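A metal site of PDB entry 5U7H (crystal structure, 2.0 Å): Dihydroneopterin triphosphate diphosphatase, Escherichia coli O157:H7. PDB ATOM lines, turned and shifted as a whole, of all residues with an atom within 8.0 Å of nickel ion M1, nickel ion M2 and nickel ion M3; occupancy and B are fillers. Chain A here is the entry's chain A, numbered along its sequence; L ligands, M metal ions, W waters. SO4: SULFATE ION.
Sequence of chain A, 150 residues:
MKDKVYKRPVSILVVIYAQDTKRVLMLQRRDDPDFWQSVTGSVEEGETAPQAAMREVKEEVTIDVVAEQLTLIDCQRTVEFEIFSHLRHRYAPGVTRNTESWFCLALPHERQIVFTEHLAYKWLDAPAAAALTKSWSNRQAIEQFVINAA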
ATOM      1  N   LYS A   7     -23.201  -8.680 -15.590  1.00  0.00           N
ATOM      2  CA  LYS A   7     -21.807  -8.723 -16.012  1.00  0.00           C
ATOM      3  C   LYS A   7     -21.161  -9.994 -15.493  1.00  0.00           C
ATOM      4  O   LYS A   7     -21.544 -10.537 -14.462  1.00  0.00           O
ATOM      5  CB  LYS A   7     -21.034  -7.510 -15.503  1.00  0.00           C
ATOM      6  CG  LYS A   7     -21.377  -6.199 -16.192  1.00  0.00           C
ATOM      7  CD  LYS A   7     -20.579  -5.020 -15.650  1.00  0.00           C
ATOM      8  CE  LYS A   7     -19.112  -5.091 -16.065  1.00  0.00           C
ATOM      9  NZ  LYS A   7     -18.977  -5.303 -17.550  1.00  0.00           N
ATOM     10  N   ILE A  12     -11.020  -8.572 -18.742  1.00  0.00           N
ATOM     11  CA  ILE A  12      -9.708  -8.260 -19.276  1.00  0.00           C
ATOM     12  C   ILE A  12      -9.447  -6.770 -19.074  1.00  0.00           C
ATOM     13  O   ILE A  12     -10.353  -5.971 -18.857  1.00  0.00           O
ATOM     14  CB  ILE A  12      -9.580  -8.627 -20.776  1.00  0.00           C
ATOM     15  CG1 ILE A  12     -10.728  -8.016 -21.579  1.00  0.00           C
ATOM     16  CG2 ILE A  12      -9.565 -10.132 -20.934  1.00  0.00           C
ATOM     17  CD1 ILE A  12     -10.454  -6.640 -22.147  1.00  0.00           C
ATOM     18  N   LEU A  27      -9.915   6.669 -20.374  1.00  0.00           N
ATOM     19  CA  LEU A  27     -11.304   6.819 -20.788  1.00  0.00           C
ATOM     20  C   LEU A  27     -12.170   7.013 -19.551  1.00  0.00           C
ATOM     21  O   LEU A  27     -11.960   6.357 -18.538  1.00  0.00           O
ATOM     22  CB  LEU A  27     -11.763   5.591 -21.584  1.00  0.00           C
ATOM     23  CG  LEU A  27     -10.850   5.104 -22.718  1.00  0.00           C
ATOM     24  CD1 LEU A  27     -11.210   3.686 -23.123  1.00  0.00           C
ATOM     25  CD2 LEU A  27     -10.969   6.024 -23.903  1.00  0.00           C
ATOM     26  N   ARG A  29     -15.492   6.767 -17.458  1.00  0.00           N
ATOM     27  CA  ARG A  29     -16.669   5.905 -17.409  1.00  0.00           C
ATOM     28  C   ARG A  29     -17.957   6.722 -17.339  1.00  0.00           C
ATOM     29  O   ARG A  29     -17.983   7.861 -16.874  1.00  0.00           O
ATOM     30  CB  ARG A  29     -16.576   4.957 -16.206  1.00  0.00           C
ATOM     31  CG  ARG A  29     -15.560   3.836 -16.385  1.00  0.00           C
ATOM     32  CD  ARG A  29     -15.800   2.739 -15.357  1.00  0.00           C
ATOM     33  NE  ARG A  29     -17.032   2.006 -15.618  1.00  0.00           N
ATOM     34  CZ  ARG A  29     -17.161   1.114 -16.599  1.00  0.00           C
ATOM     35  NH1 ARG A  29     -16.136   0.832 -17.397  1.00  0.00           N
ATOM     36  NH2 ARG A  29     -18.318   0.477 -16.771  1.00  0.00           N
ATOM     37  N   GLN A  37     -10.130   5.125 -16.899  1.00  0.00           N
ATOM     38  CA  GLN A  37      -9.545   3.792 -17.020  1.00  0.00           C
ATOM     39  C   GLN A  37      -8.963   3.557 -18.406  1.00  0.00           C
ATOM     40  O   GLN A  37      -9.280   4.263 -19.369  1.00  0.00           O
ATOM     41  CB  GLN A  37     -10.595   2.724 -16.765  1.00  0.00           C
ATOM     42  CG  GLN A  37     -11.825   2.884 -17.649  1.00  0.00           C
ATOM     43  CD  GLN A  37     -12.703   1.643 -17.631  1.00  0.00           C
ATOM     44  OE1 GLN A  37     -13.761   1.598 -18.278  1.00  0.00           O
ATOM     45  NE2 GLN A  37     -12.278   0.632 -16.883  1.00  0.00           N
ATOM     46  N   SER A  38      -8.108   2.544 -18.488  1.00  0.00           N
ATOM     47  CA  SER A  38      -7.847   1.854 -19.742  1.00  0.00           C
ATOM     48  C   SER A  38      -9.081   1.050 -20.159  1.00  0.00           C
ATOM     49  O   SER A  38     -10.108   1.060 -19.493  1.00  0.00           O
ATOM     50  CB  SER A  38      -6.633   0.920 -19.591  1.00  0.00           C
ATOM     51  OG  SER A  38      -5.507   1.594 -19.040  1.00  0.00           O
ATOM     52  N   VAL A  39      -8.972   0.329 -21.258  1.00  0.00           N
ATOM     53  CA  VAL A  39     -10.085  -0.506 -21.716  1.00  0.00           C
ATOM     54  C   VAL A  39     -10.216  -1.718 -20.794  1.00  0.00           C
ATOM     55  O   VAL A  39      -9.273  -2.499 -20.625  1.00  0.00           O
ATOM     56  CB  VAL A  39      -9.878  -0.946 -23.170  1.00  0.00           C
ATOM     57  CG1 VAL A  39     -10.851  -2.017 -23.566  1.00  0.00           C
ATOM     58  CG2 VAL A  39     -10.008   0.254 -24.124  1.00  0.00           C
ATOM     59  N   THR A  40     -11.396  -1.888 -20.178  1.00  0.00           N
ATOM     60  CA  THR A  40     -11.733  -3.166 -19.547  1.00  0.00           C
ATOM     61  C   THR A  40     -13.019  -3.699 -20.133  1.00  0.00           C
ATOM     62  O   THR A  40     -13.797  -2.964 -20.741  1.00  0.00           O
ATOM     63  CB  THR A  40     -11.855  -3.065 -18.015  1.00  0.00           C
ATOM     64  OG1 THR A  40     -13.070  -2.376 -17.663  1.00  0.00           O
ATOM     65  CG2 THR A  40     -10.663  -2.343 -17.429  1.00  0.00           C
ATOM     66  N   GLY A  41     -13.236  -5.014 -19.962  1.00  0.00           N
ATOM     67  CA  GLY A  41     -14.460  -5.649 -20.399  1.00  0.00           C
ATOM     68  C   GLY A  41     -14.638  -7.080 -19.897  1.00  0.00           C
ATOM     69  O   GLY A  41     -13.651  -7.784 -19.633  1.00  0.00           O
ATOM     70  N   SER A  42     -15.890  -7.503 -19.761  1.00  0.00           N
ATOM     71  CA  SER A  42     -16.159  -8.868 -19.320  1.00  0.00           C
ATOM     72  C   SER A  42     -15.816  -9.845 -20.434  1.00  0.00           C
ATOM     73  O   SER A  42     -16.079  -9.593 -21.607  1.00  0.00           O
ATOM     74  CB  SER A  42     -17.635  -9.046 -18.922  1.00  0.00           C
ATOM     75  OG  SER A  42     -17.908  -8.373 -17.705  1.00  0.00           O
ATOM     76  N   VAL A  43     -15.204 -10.964 -20.052  1.00  0.00           N
ATOM     77  CA  VAL A  43     -15.037 -12.093 -20.973  1.00  0.00           C
ATOM     78  C   VAL A  43     -16.357 -12.844 -21.054  1.00  0.00           C
ATOM     79  O   VAL A  43     -16.899 -13.270 -20.026  1.00  0.00           O
ATOM     80  CB  VAL A  43     -13.900 -13.012 -20.517  1.00  0.00           C
ATOM     81  CG1 VAL A  43     -13.763 -14.178 -21.493  1.00  0.00           C
ATOM     82  CG2 VAL A  43     -12.591 -12.226 -20.362  1.00  0.00           C
ATOM     83  N   GLU A  44     -16.871 -13.029 -22.262  1.00  0.00           N
ATOM     84  CA  GLU A  44     -18.153 -13.704 -22.442  1.00  0.00           C
ATOM     85  C   GLU A  44     -17.976 -15.207 -22.580  1.00  0.00           C
ATOM     86  O   GLU A  44     -16.897 -15.710 -22.913  1.00  0.00           O
ATOM     87  CB  GLU A  44     -18.900 -13.164 -23.671  1.00  0.00           C
ATOM     88  CG  GLU A  44     -18.969 -11.637 -23.783  1.00  0.00           C
ATOM     89  CD  GLU A  44     -20.024 -10.996 -22.889  1.00  0.00           C
ATOM     90  OE1 GLU A  44     -20.607 -11.703 -22.037  1.00  0.00           O
ATOM     91  OE2 GLU A  44     -20.275  -9.785 -23.030  1.00  0.00           O
ATOM     92  N   GLU A  47     -15.698 -17.428 -25.164  1.00  0.00           N
ATOM     93  CA  GLU A  47     -14.586 -16.685 -25.737  1.00  0.00           C
ATOM     94  C   GLU A  47     -13.406 -16.672 -24.776  1.00  0.00           C
ATOM     95  O   GLU A  47     -13.569 -16.737 -23.545  1.00  0.00           O
ATOM     96  CB  GLU A  47     -14.995 -15.246 -26.147  1.00  0.00           C
ATOM     97  CG  GLU A  47     -14.990 -14.203 -25.036  1.00  0.00           C
ATOM     98  CD  GLU A  47     -15.383 -12.807 -25.534  1.00  0.00           C
ATOM     99  OE1 GLU A  47     -15.088 -12.458 -26.699  1.00  0.00           O
ATOM    100  OE2 GLU A  47     -16.004 -12.065 -24.736  1.00  0.00           O
ATOM    101  N   ALA A  52     -11.597 -11.616 -26.053  1.00  0.00           N
ATOM    102  CA  ALA A  52     -12.359 -10.551 -25.416  1.00  0.00           C
ATOM    103  C   ALA A  52     -11.595  -9.236 -25.467  1.00  0.00           C
ATOM    104  O   ALA A  52     -12.181  -8.161 -25.653  1.00  0.00           O
ATOM    105  CB  ALA A  52     -12.686 -10.914 -23.983  1.00  0.00           C
ATOM    106  N   ARG A  55     -12.026  -7.865 -28.932  1.00  0.00           N
ATOM    107  CA  ARG A  55     -13.408  -7.421 -29.148  1.00  0.00           C
ATOM    108  C   ARG A  55     -13.675  -6.105 -28.434  1.00  0.00           C
ATOM    109  O   ARG A  55     -14.185  -5.155 -29.027  1.00  0.00           O
ATOM    110  CB  ARG A  55     -14.389  -8.497 -28.707  1.00  0.00           C
ATOM    111  CG  ARG A  55     -15.843  -8.084 -28.921  1.00  0.00           C
ATOM    112  CD  ARG A  55     -16.843  -9.087 -28.360  1.00  0.00           C
ATOM    113  NE  ARG A  55     -16.462  -9.615 -27.066  1.00  0.00           N
ATOM    114  CZ  ARG A  55     -16.470  -8.919 -25.930  1.00  0.00           C
ATOM    115  NH1 ARG A  55     -16.873  -7.657 -25.908  1.00  0.00           N
ATOM    116  NH2 ARG A  55     -16.078  -9.509 -24.818  1.00  0.00           N
ATOM    117  N   GLU A  56     -13.312  -6.027 -27.134  1.00  0.00           N
ATOM    118  CA  GLU A  56     -13.559  -4.805 -26.386  1.00  0.00           C
ATOM    119  C   GLU A  56     -12.742  -3.633 -26.924  1.00  0.00           C
ATOM    120  O   GLU A  56     -13.207  -2.490 -26.900  1.00  0.00           O
ATOM    121  CB  GLU A  56     -13.263  -5.036 -24.904  1.00  0.00           C
ATOM    122  CG  GLU A  56     -14.256  -5.984 -24.224  1.00  0.00           C
ATOM    123  CD  GLU A  56     -15.621  -5.358 -23.904  1.00  0.00           C
ATOM    124  OE1 GLU A  56     -15.747  -4.119 -23.888  1.00  0.00           O
ATOM    125  OE2 GLU A  56     -16.570  -6.135 -23.640  1.00  0.00           O
ATOM    126  N   VAL A  57     -11.525  -3.870 -27.412  1.00  0.00           N
ATOM    127  CA  VAL A  57     -10.781  -2.761 -28.001  1.00  0.00           C
ATOM    128  C   VAL A  57     -11.511  -2.222 -29.229  1.00  0.00           C
ATOM    129  O   VAL A  57     -11.626  -0.998 -29.413  1.00  0.00           O
ATOM    130  CB  VAL A  57      -9.335  -3.186 -28.342  1.00  0.00           C
ATOM    131  CG1 VAL A  57      -8.645  -2.124 -29.214  1.00  0.00           C
ATOM    132  CG2 VAL A  57      -8.539  -3.400 -27.039  1.00  0.00           C
ATOM    133  N   GLU A  59     -14.809  -2.499 -29.845  1.00  0.00           N
ATOM    134  CA  GLU A  59     -16.051  -1.881 -29.379  1.00  0.00           C
ATOM    135  C   GLU A  59     -15.796  -0.518 -28.741  1.00  0.00           C
ATOM    136  O   GLU A  59     -16.425   0.474 -29.100  1.00  0.00           O
ATOM    137  CB  GLU A  59     -16.750  -2.794 -28.373  1.00  0.00           C
ATOM    138  CG  GLU A  59     -17.314  -4.088 -28.945  1.00  0.00           C
ATOM    139  CD  GLU A  59     -17.927  -5.002 -27.872  1.00  0.00           C
ATOM    140  OE1 GLU A  59     -17.863  -4.653 -26.658  1.00  0.00           O
ATOM    141  OE2 GLU A  59     -18.454  -6.067 -28.244  1.00  0.00           O
ATOM    142  N   GLU A  60     -14.849  -0.443 -27.797  1.00  0.00           N
ATOM    143  CA  GLU A  60     -14.716   0.716 -26.934  1.00  0.00           C
ATOM    144  C   GLU A  60     -13.916   1.860 -27.553  1.00  0.00           C
ATOM    145  O   GLU A  60     -14.196   3.024 -27.258  1.00  0.00           O
ATOM    146  CB  GLU A  60     -14.078   0.292 -25.613  1.00  0.00           C
ATOM    147  CG  GLU A  60     -14.908  -0.760 -24.901  1.00  0.00           C
ATOM    148  CD  GLU A  60     -14.698  -0.785 -23.418  1.00  0.00           C
ATOM    149  OE1 GLU A  60     -13.824  -0.035 -22.941  1.00  0.00           O
ATOM    150  OE2 GLU A  60     -15.421  -1.552 -22.726  1.00  0.00           O
ATOM    151  N   VAL A  61     -12.902   1.585 -28.372  1.00  0.00           N
ATOM    152  CA  VAL A  61     -12.118   2.693 -28.938  1.00  0.00           C
ATOM    153  C   VAL A  61     -11.992   2.570 -30.451  1.00  0.00           C
ATOM    154  O   VAL A  61     -11.157   3.245 -31.062  1.00  0.00           O
ATOM    155  CB  VAL A  61     -10.719   2.798 -28.274  1.00  0.00           C
ATOM    156  CG1 VAL A  61     -10.860   3.077 -26.783  1.00  0.00           C
ATOM    157  CG2 VAL A  61      -9.862   1.554 -28.533  1.00  0.00           C
ATOM    158  N   ARG A  90     -24.390  -4.760 -10.779  1.00  0.00           N
ATOM    159  CA  ARG A  90     -24.408  -5.293 -12.129  1.00  0.00           C
ATOM    160  C   ARG A  90     -23.976  -6.767 -12.197  1.00  0.00           C
ATOM    161  O   ARG A  90     -23.976  -7.342 -13.294  1.00  0.00           O
ATOM    162  CB  ARG A  90     -23.520  -4.438 -13.034  1.00  0.00           C
ATOM    163  CG  ARG A  90     -24.125  -3.056 -13.285  1.00  0.00           C
ATOM    164  CD  ARG A  90     -25.189  -3.119 -14.382  1.00  0.00           C
ATOM    165  NE  ARG A  90     -24.565  -3.323 -15.692  1.00  0.00           N
ATOM    166  CZ  ARG A  90     -24.755  -4.382 -16.470  1.00  0.00           C
ATOM    167  NH1 ARG A  90     -25.580  -5.350 -16.085  1.00  0.00           N
ATOM    168  NH2 ARG A  90     -24.137  -4.459 -17.641  1.00  0.00           N
ATOM    169  N   THR A 116     -17.408   4.642 -27.456  1.00  0.00           N
ATOM    170  CA  THR A 116     -18.825   4.318 -27.310  1.00  0.00           C
ATOM    171  C   THR A 116     -19.287   4.086 -25.878  1.00  0.00           C
ATOM    172  O   THR A 116     -20.415   4.432 -25.540  1.00  0.00           O
ATOM    173  CB  THR A 116     -19.185   3.094 -28.146  1.00  0.00           C
ATOM    174  OG1 THR A 116     -18.414   1.959 -27.695  1.00  0.00           O
ATOM    175  CG2 THR A 116     -18.889   3.335 -29.612  1.00  0.00           C
ATOM    176  N   GLU A 117     -18.439   3.515 -25.018  1.00  0.00           N
ATOM    177  CA  GLU A 117     -18.798   3.173 -23.648  1.00  0.00           C
ATOM    178  C   GLU A 117     -18.437   4.271 -22.647  1.00  0.00           C
ATOM    179  O   GLU A 117     -18.706   4.109 -21.442  1.00  0.00           O
ATOM    180  CB  GLU A 117     -18.099   1.849 -23.267  1.00  0.00           C
ATOM    181  CG  GLU A 117     -18.481   1.169 -21.922  1.00  0.00           C
ATOM    182  CD  GLU A 117     -17.695  -0.138 -21.707  1.00  0.00           C
ATOM    183  OE1 GLU A 117     -16.786  -0.188 -20.804  1.00  0.00           O
ATOM    184  OE2 GLU A 117     -17.987  -1.096 -22.459  1.00  0.00           O
ATOM    185  N   HIS A 118     -17.870   5.393 -23.092  1.00  0.00           N
ATOM    186  CA  HIS A 118     -17.292   6.357 -22.180  1.00  0.00           C
ATOM    187  C   HIS A 118     -17.776   7.758 -22.517  1.00  0.00           C
ATOM    188  O   HIS A 118     -18.411   7.990 -23.543  1.00  0.00           O
ATOM    189  CB  HIS A 118     -15.744   6.273 -22.216  1.00  0.00           C
ATOM    190  CG  HIS A 118     -15.204   4.993 -21.638  1.00  0.00           C
ATOM    191  ND1 HIS A 118     -15.121   3.825 -22.373  1.00  0.00           N
ATOM    192  CD2 HIS A 118     -14.768   4.687 -20.392  1.00  0.00           C
ATOM    193  CE1 HIS A 118     -14.634   2.862 -21.612  1.00  0.00           C
ATOM    194  NE2 HIS A 118     -14.401   3.357 -20.400  1.00  0.00           N
HETATM  195  S   SO4 L   1     -17.684  -3.991 -20.260  1.00  0.00           S
HETATM  196  O1  SO4 L   1     -17.217  -4.090 -18.881  1.00  0.00           O
HETATM  197  O2  SO4 L   1     -19.042  -3.407 -20.285  1.00  0.00           O
HETATM  198  O3  SO4 L   1     -16.770  -3.128 -21.057  1.00  0.00           O
HETATM  199  O4  SO4 L   1     -17.734  -5.317 -20.859  1.00  0.00           O
HETATM  200 NI    NI M   1     -16.980  -2.751 -23.084  1.00  0.00          NI
HETATM  201 NI    NI M   2     -15.334  -1.756 -20.723  1.00  0.00          NI
HETATM  202 NI    NI M   3     -18.329  -5.903 -22.668  1.00  0.00          NI
HETATM  203 NI    NI M   4     -20.181  -3.533 -21.959  1.00  0.00          NI
HETATM  204  O   HOH W   1     -18.300  -8.045 -22.408  1.00  0.00           O
HETATM  205  O   HOH W   2     -18.577  -4.014 -23.336  1.00  0.00           O
HETATM  206  O   HOH W   3     -20.431  -5.704 -21.974  1.00  0.00           O
HETATM  207  O   HOH W   4     -17.462  -2.498 -25.118  1.00  0.00           O
HETATM  208  O   HOH W   5     -15.405  -1.773 -18.738  1.00  0.00           O
HETATM  209  O   HOH W   6     -19.030  -6.376 -24.506  1.00  0.00           O
HETATM  210  O   HOH W   7     -13.827  -0.424 -20.376  1.00  0.00           O
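Nickel ion M2 is bound by O of Thr 40 (2.0 Å), water W5 (2.0 Å), O3 of the ligand (2.0 Å), OE2 of Glu 60 (2.0 Å), water W7 (2.0 Å) and OE1 of Glu 117 (2.1 Å).
Water W5 lies within hydrogen-bond range of OG1 of Thr 40 (2.6 Å) and NH1 of Arg 29 (3.0 Å).
Water W7 lies within hydrogen-bond range of the side-chain carboxylate (OE1) of Glu 60 (2.6 Å), the backbone NH (N) of Thr 40 (2.8 Å) and the side-chain amide oxygen (OE1) of Gln 37 (2.9 Å).
Water W6 lies within hydrogen-bond range of NH1 of Arg 55 (2.9 Å) and OE1 of Glu 59 (3.0 Å).
Water W1 bridges OE2 of Glu 44 and O of Ser 42.
Nickel ion M3 is bound by an oxygen (O4) of the ligand, water W2, water W6, the side-chain carboxylate of Glu 56, water W1 and water W3.
Nickel ion M1 is bound by OE2 of Glu 60, OE1 of Glu 56, OE2 of Glu 117, water W2, O3 of the ligand and water W4.
OG1 of Thr 40 sits at hydrogen-bond distance from NE2 of Gln 37 (3.2 Å).
The side-chain carboxylate (OE2) of Glu 56 lies close to the guanidinium group (NH1) of Arg 55 (2.7 Å).
The side-chain carboxylate of Glu 117 lies close to the guanidinium group of Arg 29 (3.6 Å).
The backbone carbonyl oxygen of Gly 41 lies within hydrogen-bond range of the backbone NH of Ile 12, at 2.9 Å.
The guanidinium group (NH2) of Arg 55 lies within hydrogen-bond range of the backbone carbonyl oxygen (O) of Ser 42.
The side-chain carboxylate (OE2) of Glu 59 lies within salt-bridge range of the guanidinium group (NH1) of Arg 55 (3.2 Å).
NH2 of Arg 55 is in salt-bridge range of OE2 of Glu 47 (2.6 Å).
Residues that only touch nickel ion M3: Arg 55 (3.96 Å).
Two residues have an atom within 4 Å of nickel ion M3: Arg 55 and Glu 56.
Of the 24 residues printed, 4 come within 4 Å of nickel ion M1.
Gly 41 touches nickel ion M2.
Within 4 Å of nickel ion M2: Thr 40, Gly 41, Glu 56, Glu 60 and Glu 117.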
